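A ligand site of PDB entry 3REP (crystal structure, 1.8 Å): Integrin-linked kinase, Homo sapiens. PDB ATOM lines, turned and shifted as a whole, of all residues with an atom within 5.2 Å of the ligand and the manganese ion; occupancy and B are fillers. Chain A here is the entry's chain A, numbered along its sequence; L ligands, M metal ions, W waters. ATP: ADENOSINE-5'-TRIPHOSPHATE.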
ATOM      1  N   LEU A  18      17.572  13.034 -15.524  1.00  0.00           N
ATOM      2  CA  LEU A  18      16.636  14.142 -15.646  1.00  0.00           C
ATOM      3  C   LEU A  18      15.688  14.269 -14.470  1.00  0.00           C
ATOM      4  O   LEU A  18      15.271  15.356 -14.112  1.00  0.00           O
ATOM      5  CB  LEU A  18      15.834  13.994 -16.952  1.00  0.00           C
ATOM      6  CG  LEU A  18      16.582  13.982 -18.284  1.00  0.00           C
ATOM      7  CD1 LEU A  18      15.567  13.741 -19.416  1.00  0.00           C
ATOM      8  CD2 LEU A  18      17.371  15.283 -18.519  1.00  0.00           C
ATOM      9  N   ASN A  19      15.346  13.143 -13.840  1.00  0.00           N
ATOM     10  CA  ASN A  19      14.350  13.134 -12.787  1.00  0.00           C
ATOM     11  C   ASN A  19      14.392  11.807 -12.028  1.00  0.00           C
ATOM     12  O   ASN A  19      14.796  10.771 -12.591  1.00  0.00           O
ATOM     13  CB  ASN A  19      12.916  13.418 -13.374  1.00  0.00           C
ATOM     14  CG  ASN A  19      11.877  13.723 -12.295  1.00  0.00           C
ATOM     15  OD1 ASN A  19      12.177  14.423 -11.291  1.00  0.00           O
ATOM     16  ND2 ASN A  19      10.657  13.189 -12.459  1.00  0.00           N
ATOM     17  N   ASN A  21      11.321  10.080  -9.243  1.00  0.00           N
ATOM     18  CA  ASN A  21      10.009  10.316  -8.639  1.00  0.00           C
ATOM     19  C   ASN A  21       9.362   9.014  -8.221  1.00  0.00           C
ATOM     20  O   ASN A  21      10.024   7.967  -8.242  1.00  0.00           O
ATOM     21  CB  ASN A  21       9.116  11.148  -9.578  1.00  0.00           C
ATOM     22  CG  ASN A  21       8.654  10.361 -10.798  1.00  0.00           C
ATOM     23  OD1 ASN A  21       9.114   9.251 -11.027  1.00  0.00           O
ATOM     24  ND2 ASN A  21       7.779  10.962 -11.614  1.00  0.00           N
ATOM     25  N   HIS A  22       8.076   9.067  -7.905  1.00  0.00           N
ATOM     26  CA  HIS A  22       7.267   7.898  -7.520  1.00  0.00           C
ATOM     27  C   HIS A  22       7.355   6.726  -8.523  1.00  0.00           C
ATOM     28  O   HIS A  22       7.293   5.567  -8.124  1.00  0.00           O
ATOM     29  CB  HIS A  22       5.794   8.306  -7.315  1.00  0.00           C
ATOM     30  CG  HIS A  22       5.209   9.064  -8.463  1.00  0.00           C
ATOM     31  ND1 HIS A  22       5.223  10.447  -8.519  1.00  0.00           N
ATOM     32  CD2 HIS A  22       4.578   8.652  -9.589  1.00  0.00           C
ATOM     33  CE1 HIS A  22       4.652  10.853  -9.638  1.00  0.00           C
ATOM     34  NE2 HIS A  22       4.248   9.781 -10.304  1.00  0.00           N
ATOM     35  N   SER A  23       7.516   7.032  -9.814  1.00  0.00           N
ATOM     36  CA  SER A  23       7.569   5.994 -10.873  1.00  0.00           C
ATOM     37  C   SER A  23       8.918   5.274 -10.987  1.00  0.00           C
ATOM     38  O   SER A  23       8.992   4.184 -11.519  1.00  0.00           O
ATOM     39  CB  SER A  23       7.307   6.635 -12.254  1.00  0.00           C
ATOM     40  OG  SER A  23       5.958   7.114 -12.344  1.00  0.00           O
ATOM     41  N   GLU A  25      12.831   6.544 -12.416  1.00  0.00           N
ATOM     42  CA  GLU A  25      13.685   7.639 -12.911  1.00  0.00           C
ATOM     43  C   GLU A  25      13.682   7.808 -14.404  1.00  0.00           C
ATOM     44  O   GLU A  25      13.281   6.896 -15.162  1.00  0.00           O
ATOM     45  CB  GLU A  25      15.140   7.514 -12.404  1.00  0.00           C
ATOM     46  CG  GLU A  25      15.688   6.156 -12.401  1.00  0.00           C
ATOM     47  CD  GLU A  25      17.089   6.025 -11.711  1.00  0.00           C
ATOM     48  OE1 GLU A  25      17.229   6.156 -10.469  1.00  0.00           O
ATOM     49  OE2 GLU A  25      18.032   5.708 -12.443  1.00  0.00           O
ATOM     50  N   LEU A  26      14.133   8.986 -14.816  1.00  0.00           N
ATOM     51  CA  LEU A  26      14.264   9.355 -16.216  1.00  0.00           C
ATOM     52  C   LEU A  26      15.643   9.916 -16.491  1.00  0.00           C
ATOM     53  O   LEU A  26      16.144  10.810 -15.772  1.00  0.00           O
ATOM     54  CB  LEU A  26      13.203  10.382 -16.625  1.00  0.00           C
ATOM     55  CG  LEU A  26      13.039  10.584 -18.145  1.00  0.00           C
ATOM     56  CD1 LEU A  26      12.219   9.435 -18.765  1.00  0.00           C
ATOM     57  CD2 LEU A  26      12.332  11.944 -18.500  1.00  0.00           C
ATOM     58  N   VAL A  37      15.056   9.442 -24.212  1.00  0.00           N
ATOM     59  CA  VAL A  37      14.991   9.379 -22.784  1.00  0.00           C
ATOM     60  C   VAL A  37      14.711   7.927 -22.422  1.00  0.00           C
ATOM     61  O   VAL A  37      14.099   7.203 -23.189  1.00  0.00           O
ATOM     62  CB  VAL A  37      13.931  10.297 -22.167  1.00  0.00           C
ATOM     63  CG1 VAL A  37      14.305  11.762 -22.453  1.00  0.00           C
ATOM     64  CG2 VAL A  37      12.563   9.964 -22.711  1.00  0.00           C
ATOM     65  N   LYS A  39      13.113   5.721 -19.461  1.00  0.00           N
ATOM     66  CA  LYS A  39      12.290   5.648 -18.261  1.00  0.00           C
ATOM     67  C   LYS A  39      12.501   4.317 -17.519  1.00  0.00           C
ATOM     68  O   LYS A  39      12.202   3.227 -18.040  1.00  0.00           O
ATOM     69  CB  LYS A  39      10.811   5.795 -18.641  1.00  0.00           C
ATOM     70  CG  LYS A  39       9.900   5.729 -17.453  1.00  0.00           C
ATOM     71  CD  LYS A  39       9.923   7.022 -16.721  1.00  0.00           C
ATOM     72  CE  LYS A  39       8.635   7.186 -15.878  1.00  0.00           C
ATOM     73  NZ  LYS A  39       8.637   8.541 -15.320  1.00  0.00           N
ATOM     74  N   LEU A  70       3.728  10.019 -30.087  1.00  0.00           N
ATOM     75  CA  LEU A  70       5.135   9.766 -29.860  1.00  0.00           C
ATOM     76  C   LEU A  70       5.285   8.310 -29.397  1.00  0.00           C
ATOM     77  O   LEU A  70       4.967   7.966 -28.235  1.00  0.00           O
ATOM     78  CB  LEU A  70       5.734  10.763 -28.849  1.00  0.00           C
ATOM     79  CG  LEU A  70       7.235  10.593 -28.538  1.00  0.00           C
ATOM     80  CD1 LEU A  70       8.057  11.038 -29.784  1.00  0.00           C
ATOM     81  CD2 LEU A  70       7.588  11.389 -27.248  1.00  0.00           C
ATOM     82  N   THR A  88      12.062   6.289 -25.422  1.00  0.00           N
ATOM     83  CA  THR A  88      11.347   7.118 -26.372  1.00  0.00           C
ATOM     84  C   THR A  88      12.264   8.238 -26.850  1.00  0.00           C
ATOM     85  O   THR A  88      13.304   8.557 -26.202  1.00  0.00           O
ATOM     86  CB  THR A  88       9.987   7.658 -25.770  1.00  0.00           C
ATOM     87  OG1 THR A  88       9.152   8.125 -26.818  1.00  0.00           O
ATOM     88  CG2 THR A  88      10.214   8.775 -24.790  1.00  0.00           C
ATOM     89  N   HIS A  89      11.929   8.805 -28.010  1.00  0.00           N
ATOM     90  CA  HIS A  89      12.737   9.903 -28.561  1.00  0.00           C
ATOM     91  C   HIS A  89      12.807  11.093 -27.608  1.00  0.00           C
ATOM     92  O   HIS A  89      11.848  11.381 -26.874  1.00  0.00           O
ATOM     93  CB  HIS A  89      12.260  10.281 -29.978  1.00  0.00           C
ATOM     94  CG  HIS A  89      12.906   9.465 -31.043  1.00  0.00           C
ATOM     95  ND1 HIS A  89      12.196   8.788 -32.014  1.00  0.00           N
ATOM     96  CD2 HIS A  89      14.219   9.200 -31.280  1.00  0.00           C
ATOM     97  CE1 HIS A  89      13.036   8.149 -32.810  1.00  0.00           C
ATOM     98  NE2 HIS A  89      14.267   8.382 -32.379  1.00  0.00           N
ATOM     99  N   TRP A  90      13.973  11.732 -27.548  1.00  0.00           N
ATOM    100  CA  TRP A  90      14.127  12.934 -26.769  1.00  0.00           C
ATOM    101  C   TRP A  90      13.449  14.101 -27.506  1.00  0.00           C
ATOM    102  O   TRP A  90      13.692  14.311 -28.699  1.00  0.00           O
ATOM    103  CB  TRP A  90      15.636  13.185 -26.634  1.00  0.00           C
ATOM    104  CG  TRP A  90      15.999  14.641 -26.394  1.00  0.00           C
ATOM    105  CD1 TRP A  90      16.362  15.564 -27.325  1.00  0.00           C
ATOM    106  CD2 TRP A  90      16.040  15.281 -25.127  1.00  0.00           C
ATOM    107  NE1 TRP A  90      16.629  16.757 -26.711  1.00  0.00           N
ATOM    108  CE2 TRP A  90      16.434  16.624 -25.368  1.00  0.00           C
ATOM    109  CE3 TRP A  90      15.801  14.871 -23.823  1.00  0.00           C
ATOM    110  CZ2 TRP A  90      16.584  17.546 -24.334  1.00  0.00           C
ATOM    111  CZ3 TRP A  90      15.943  15.794 -22.794  1.00  0.00           C
ATOM    112  CH2 TRP A  90      16.333  17.116 -23.049  1.00  0.00           C
ATOM    113  N   MET A  91      12.570  14.834 -26.803  1.00  0.00           N
ATOM    114  CA  MET A  91      11.823  15.957 -27.390  1.00  0.00           C
ATOM    115  C   MET A  91      12.397  17.236 -26.789  1.00  0.00           C
ATOM    116  O   MET A  91      12.337  17.443 -25.567  1.00  0.00           O
ATOM    117  CB  MET A  91      10.293  15.848 -27.110  1.00  0.00           C
ATOM    118  CG  MET A  91       9.657  14.594 -27.708  1.00  0.00           C
ATOM    119  SD  MET A  91       9.309  14.791 -29.439  1.00  0.00           S
ATOM    120  CE  MET A  91      10.550  13.748 -30.156  1.00  0.00           C
ATOM    121  N   GLY A  94      10.453  19.350 -24.332  1.00  0.00           N
ATOM    122  CA  GLY A  94       9.961  18.628 -23.172  1.00  0.00           C
ATOM    123  C   GLY A  94       8.451  18.548 -23.305  1.00  0.00           C
ATOM    124  O   GLY A  94       7.964  18.435 -24.447  1.00  0.00           O
ATOM    125  N   SER A  95       7.735  18.607 -22.173  1.00  0.00           N
ATOM    126  CA  SER A  95       6.257  18.394 -22.156  1.00  0.00           C
ATOM    127  C   SER A  95       5.533  19.685 -22.494  1.00  0.00           C
ATOM    128  O   SER A  95       6.088  20.804 -22.394  1.00  0.00           O
ATOM    129  CB  SER A  95       5.783  17.871 -20.788  1.00  0.00           C
ATOM    130  OG  SER A  95       5.980  18.890 -19.775  1.00  0.00           O
ATOM    131  N   ASN A  98       5.767  21.787 -19.453  1.00  0.00           N
ATOM    132  CA  ASN A  98       7.038  22.558 -19.425  1.00  0.00           C
ATOM    133  C   ASN A  98       6.916  23.831 -20.248  1.00  0.00           C
ATOM    134  O   ASN A  98       7.244  24.939 -19.768  1.00  0.00           O
ATOM    135  CB  ASN A  98       8.263  21.767 -19.948  1.00  0.00           C
ATOM    136  CG  ASN A  98       8.618  20.516 -19.125  1.00  0.00           C
ATOM    137  OD1 ASN A  98       8.479  20.469 -17.870  1.00  0.00           O
ATOM    138  ND2 ASN A  98       9.167  19.518 -19.821  1.00  0.00           N
ATOM    139  N   ARG A 142       1.259  17.071 -18.967  1.00  0.00           N
ATOM    140  CA  ARG A 142       2.477  16.382 -18.676  1.00  0.00           C
ATOM    141  C   ARG A 142       2.660  15.163 -19.574  1.00  0.00           C
ATOM    142  O   ARG A 142       3.783  14.692 -19.773  1.00  0.00           O
ATOM    143  CB  ARG A 142       2.507  15.960 -17.199  1.00  0.00           C
ATOM    144  CG  ARG A 142       2.942  17.121 -16.285  1.00  0.00           C
ATOM    145  CD  ARG A 142       3.625  16.566 -15.009  1.00  0.00           C
ATOM    146  NE  ARG A 142       4.437  17.595 -14.339  1.00  0.00           N
ATOM    147  CZ  ARG A 142       3.939  18.459 -13.466  1.00  0.00           C
ATOM    148  NH1 ARG A 142       2.639  18.403 -13.178  1.00  0.00           N
ATOM    149  NH2 ARG A 142       4.735  19.339 -12.860  1.00  0.00           N
ATOM    150  N   MET A 145       4.212  15.704 -25.411  1.00  0.00           N
ATOM    151  CA  MET A 145       5.563  16.308 -25.623  1.00  0.00           C
ATOM    152  C   MET A 145       5.572  17.269 -26.812  1.00  0.00           C
ATOM    153  O   MET A 145       4.786  17.120 -27.755  1.00  0.00           O
ATOM    154  CB  MET A 145       6.575  15.194 -25.874  1.00  0.00           C
ATOM    155  CG  MET A 145       6.726  14.210 -24.707  1.00  0.00           C
ATOM    156  SD  MET A 145       7.378  15.053 -23.227  1.00  0.00           S
ATOM    157  CE  MET A 145       6.366  14.222 -21.980  1.00  0.00           C
ATOM    158  N   ALA A 157       4.998   6.926 -23.761  1.00  0.00           N
ATOM    159  CA  ALA A 157       5.824   6.590 -22.580  1.00  0.00           C
ATOM    160  C   ALA A 157       5.222   7.101 -21.226  1.00  0.00           C
ATOM    161  O   ALA A 157       5.794   6.846 -20.127  1.00  0.00           O
ATOM    162  CB  ALA A 157       7.279   7.136 -22.754  1.00  0.00           C
ATOM    163  N   ASP A 158       4.120   7.851 -21.308  1.00  0.00           N
ATOM    164  CA  ASP A 158       3.382   8.283 -20.138  1.00  0.00           C
ATOM    165  C   ASP A 158       2.151   7.429 -19.794  1.00  0.00           C
ATOM    166  O   ASP A 158       1.474   7.664 -18.803  1.00  0.00           O
ATOM    167  CB  ASP A 158       3.089   9.751 -20.251  1.00  0.00           C
ATOM    168  CG  ASP A 158       4.304  10.547 -19.838  1.00  0.00           C
ATOM    169  OD1 ASP A 158       4.546  10.489 -18.625  1.00  0.00           O
ATOM    170  OD2 ASP A 158       4.993  11.133 -20.698  1.00  0.00           O
ATOM    171  N   LYS A 160       0.370   4.543 -18.074  1.00  0.00           N
ATOM    172  CA  LYS A 160       0.695   3.857 -16.841  1.00  0.00           C
ATOM    173  C   LYS A 160       0.563   2.332 -17.053  1.00  0.00           C
ATOM    174  O   LYS A 160      -0.398   1.867 -17.638  1.00  0.00           O
ATOM    175  CB  LYS A 160      -0.218   4.342 -15.710  1.00  0.00           C
ATOM    176  CG  LYS A 160       0.020   5.798 -15.325  1.00  0.00           C
ATOM    177  CD  LYS A 160       1.332   5.935 -14.493  1.00  0.00           C
ATOM    178  CE  LYS A 160       1.748   7.417 -14.255  1.00  0.00           C
ATOM    179  NZ  LYS A 160       1.927   8.214 -15.499  1.00  0.00           N
ATOM    180  N   GLN A 164       1.990  -0.033 -12.178  1.00  0.00           N
ATOM    181  CA  GLN A 164       2.696   1.255 -11.996  1.00  0.00           C
ATOM    182  C   GLN A 164       1.774   2.212 -11.238  1.00  0.00           C
ATOM    183  O   GLN A 164       0.782   2.682 -11.811  1.00  0.00           O
ATOM    184  CB  GLN A 164       3.145   1.850 -13.336  1.00  0.00           C
ATOM    185  CG  GLN A 164       4.002   3.156 -13.210  1.00  0.00           C
ATOM    186  CD  GLN A 164       4.217   3.899 -14.512  1.00  0.00           C
ATOM    187  OE1 GLN A 164       4.746   5.021 -14.515  1.00  0.00           O
ATOM    188  NE2 GLN A 164       3.773   3.322 -15.610  1.00  0.00           N
HETATM  189  PG  ATP L   1       5.470  10.019 -14.480  1.00  0.00           P
HETATM  190  O1G ATP L   1       5.599   9.686 -15.940  1.00  0.00           O
HETATM  191  O2G ATP L   1       4.112   9.566 -13.870  1.00  0.00           O
HETATM  192  O3G ATP L   1       6.586   9.188 -13.705  1.00  0.00           O
HETATM  193  PB  ATP L   1       6.342  12.738 -14.885  1.00  0.00           P
HETATM  194  O1B ATP L   1       5.989  12.654 -16.324  1.00  0.00           O
HETATM  195  O2B ATP L   1       5.934  13.945 -14.103  1.00  0.00           O
HETATM  196  O3B ATP L   1       5.730  11.574 -14.061  1.00  0.00           O
HETATM  197  PA  ATP L   1       9.007  11.952 -15.695  1.00  0.00           P
HETATM  198  O1A ATP L   1      10.153  11.551 -14.825  1.00  0.00           O
HETATM  199  O2A ATP L   1       8.369  10.969 -16.612  1.00  0.00           O
HETATM  200  O3A ATP L   1       7.910  12.583 -14.686  1.00  0.00           O
HETATM  201  O5' ATP L   1       9.411  13.203 -16.507  1.00  0.00           O
HETATM  202  C5' ATP L   1      10.324  14.184 -15.900  1.00  0.00           C
HETATM  203  C4' ATP L   1      10.640  15.301 -16.935  1.00  0.00           C
HETATM  204  O4' ATP L   1      11.329  14.723 -18.069  1.00  0.00           O
HETATM  205  C3' ATP L   1       9.362  15.864 -17.577  1.00  0.00           C
HETATM  206  O3' ATP L   1       8.836  16.950 -16.797  1.00  0.00           O
HETATM  207  C2' ATP L   1       9.850  16.395 -18.911  1.00  0.00           C
HETATM  208  O2' ATP L   1      10.441  17.703 -18.700  1.00  0.00           O
HETATM  209  C1' ATP L   1      10.953  15.404 -19.264  1.00  0.00           C
HETATM  210  N9  ATP L   1      10.550  14.442 -20.324  1.00  0.00           N
HETATM  211  C8  ATP L   1       9.680  13.418 -20.293  1.00  0.00           C
HETATM  212  N7  ATP L   1       9.681  12.814 -21.509  1.00  0.00           N
HETATM  213  C5  ATP L   1      10.532  13.468 -22.297  1.00  0.00           C
HETATM  214  C6  ATP L   1      10.981  13.340 -23.633  1.00  0.00           C
HETATM  215  N6  ATP L   1      10.536  12.401 -24.505  1.00  0.00           N
HETATM  216  N1  ATP L   1      11.898  14.209 -24.084  1.00  0.00           N
HETATM  217  C2  ATP L   1      12.399  15.153 -23.308  1.00  0.00           C
HETATM  218  N3  ATP L   1      12.024  15.335 -22.057  1.00  0.00           N
HETATM  219  C4  ATP L   1      11.089  14.487 -21.523  1.00  0.00           C
HETATM  220 MN    MN M   1       6.444  10.901 -17.553  1.00  0.00          MN
HETATM  221  O   HOH W   1       8.904   9.888 -20.737  1.00  0.00           O
HETATM  222  O   HOH W   2       6.233  17.368 -17.513  1.00  0.00           O
HETATM  223  O   HOH W   3       7.055  12.204 -19.258  1.00  0.00           O
HETATM  224  O   HOH W   4      12.332  20.122 -17.052  1.00  0.00           O
HETATM  225  O   HOH W   5       8.005  10.950 -23.088  1.00  0.00           O
HETATM  226  O   HOH W   6      13.337  17.559 -20.759  1.00  0.00           O
HETATM  227  O   HOH W   7      13.521  17.498 -17.752  1.00  0.00           O
HETATM  228  O   HOH W   8       3.992   7.456 -16.760  1.00  0.00           O
HETATM  229  O   HOH W   9       6.028  14.595 -18.239  1.00  0.00           O
HETATM  230  O   HOH W  10       2.960  11.175 -12.212  1.00  0.00           O
HETATM  231  O   HOH W  11      10.762   9.337 -13.385  1.00  0.00           O
HETATM  232  O   HOH W  12      10.500  18.745 -15.634  1.00  0.00           O
HETATM  233  O   HOH W  13       3.574  13.614 -11.940  1.00  0.00           O
HETATM  234  O   HOH W  14       7.413   8.996 -18.663  1.00  0.00           O
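The side-chain sulfur (SD) of Met 145 lies close to a nitrogen (N7) of the ligand (3.6 Å). Residues that only touch the ligand: His 22 (3.6 Å), Leu 26 (3.0 Å), Val 37 (3.6 Å), Thr 88 (3.7 Å) and Trp 90 (3.5 Å). Hydrophobic or aromatic side chains that line the ligand: Leu 26, Val 37, Trp 90, Met 91 and Met 145. Within 4 Å of the ligand: Asn 19, Asn 21, His 22, Ser 23, Leu 26, Val 37, Lys 39, Thr 88, His 89, Trp 90, Met 91, Asn 98, Arg 142, Met 145, Asp 158 and Lys 160.
Water W10 lies within hydrogen-bond range of O2G of the ligand (2.6 Å) and NE2 of His 22 (2.7 Å). Water W12 lies within hydrogen-bond range of O3' of the ligand (2.7 Å) and OD1 of Asn 98 (3.5 Å). Water W11 lies within hydrogen-bond range of O1A of the ligand, OD1 of Asn 21 and NZ of Lys 39. Water W2 bridges O3' of the ligand and OG of Ser 95. Water W8 lies within hydrogen-bond range of NZ of Lys 160 (2.5 Å), O of Asp 158 (3.2 Å) and OE1 of Gln 164 (3.4 Å).
Merely in contact with the manganese ion: Lys 39 (3.9 Å). Two residues have an atom within 4 Å of the manganese ion: Lys 39 and Asp 158.
The manganese ion is bound by O2A of the ligand. The manganese ion is bound by O1B of the ligand (2.2 Å). O1G of the ligand is bound to the manganese ion. OD1 of Asp 158 is bound to the manganese ion, 2.2 Å away. Water W3 is bound to the manganese ion. Water W14 binds the manganese ion (2.4 Å). The manganese ion has six donor atoms within binding distance.
OG of Ser 23 sits at hydrogen-bond distance from OE1 of Gln 164, at 3.3 Å. N of Val 37 is in hydrogen-bond range of O of Thr 88 (2.8 Å). The backbone NH (N) of Ser 95 sits close to the side-chain amide nitrogen (ND2) of Asn 98 (2.9 Å). The backbone NH (N) of Leu 18 is in hydrogen-bond range of the backbone carbonyl oxygen (O) of Leu 26, 2.7 Å away. O of Asn 19 lies within hydrogen-bond range of N of Leu 26, 2.9 Å away. OD1 of Asn 21 sits at hydrogen-bond distance from N of Ser 23. The backbone carbonyl oxygen of Asp 158 lies within hydrogen-bond range of the side-chain amino group of Lys 160, 3.4 Å away. The backbone NH (N) of Ser 95 lies close to the side-chain sulfur (SD) of Met 145 (3.7 Å).
N of Met 91 sits at hydrogen-bond distance from N1 of the ligand (2.9 Å). NZ of Lys 160 lies within salt-bridge range of O2G of the ligand. O3G of the ligand is in hydrogen-bond range of ND2 of Asn 21. O of His 89 sits at hydrogen-bond distance from N6 of the ligand, at 2.9 Å. The side-chain hydroxyl of Ser 23 sits at hydrogen-bond distance from an oxygen (O3G) of the ligand, 2.6 Å away. The guanidinium group of Arg 142 is in salt-bridge range of an oxygen (O2B) of the ligand. The side-chain amide nitrogen (ND2) of Asn 98 lies within hydrogen-bond range of an oxygen (O2') of the ligand, 2.5 Å away. O3G of the ligand lies within salt-bridge range of NZ of Lys 39 (2.7 Å). ND2 of Asn 19 lies within hydrogen-bond range of O1A of the ligand (2.9 Å).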
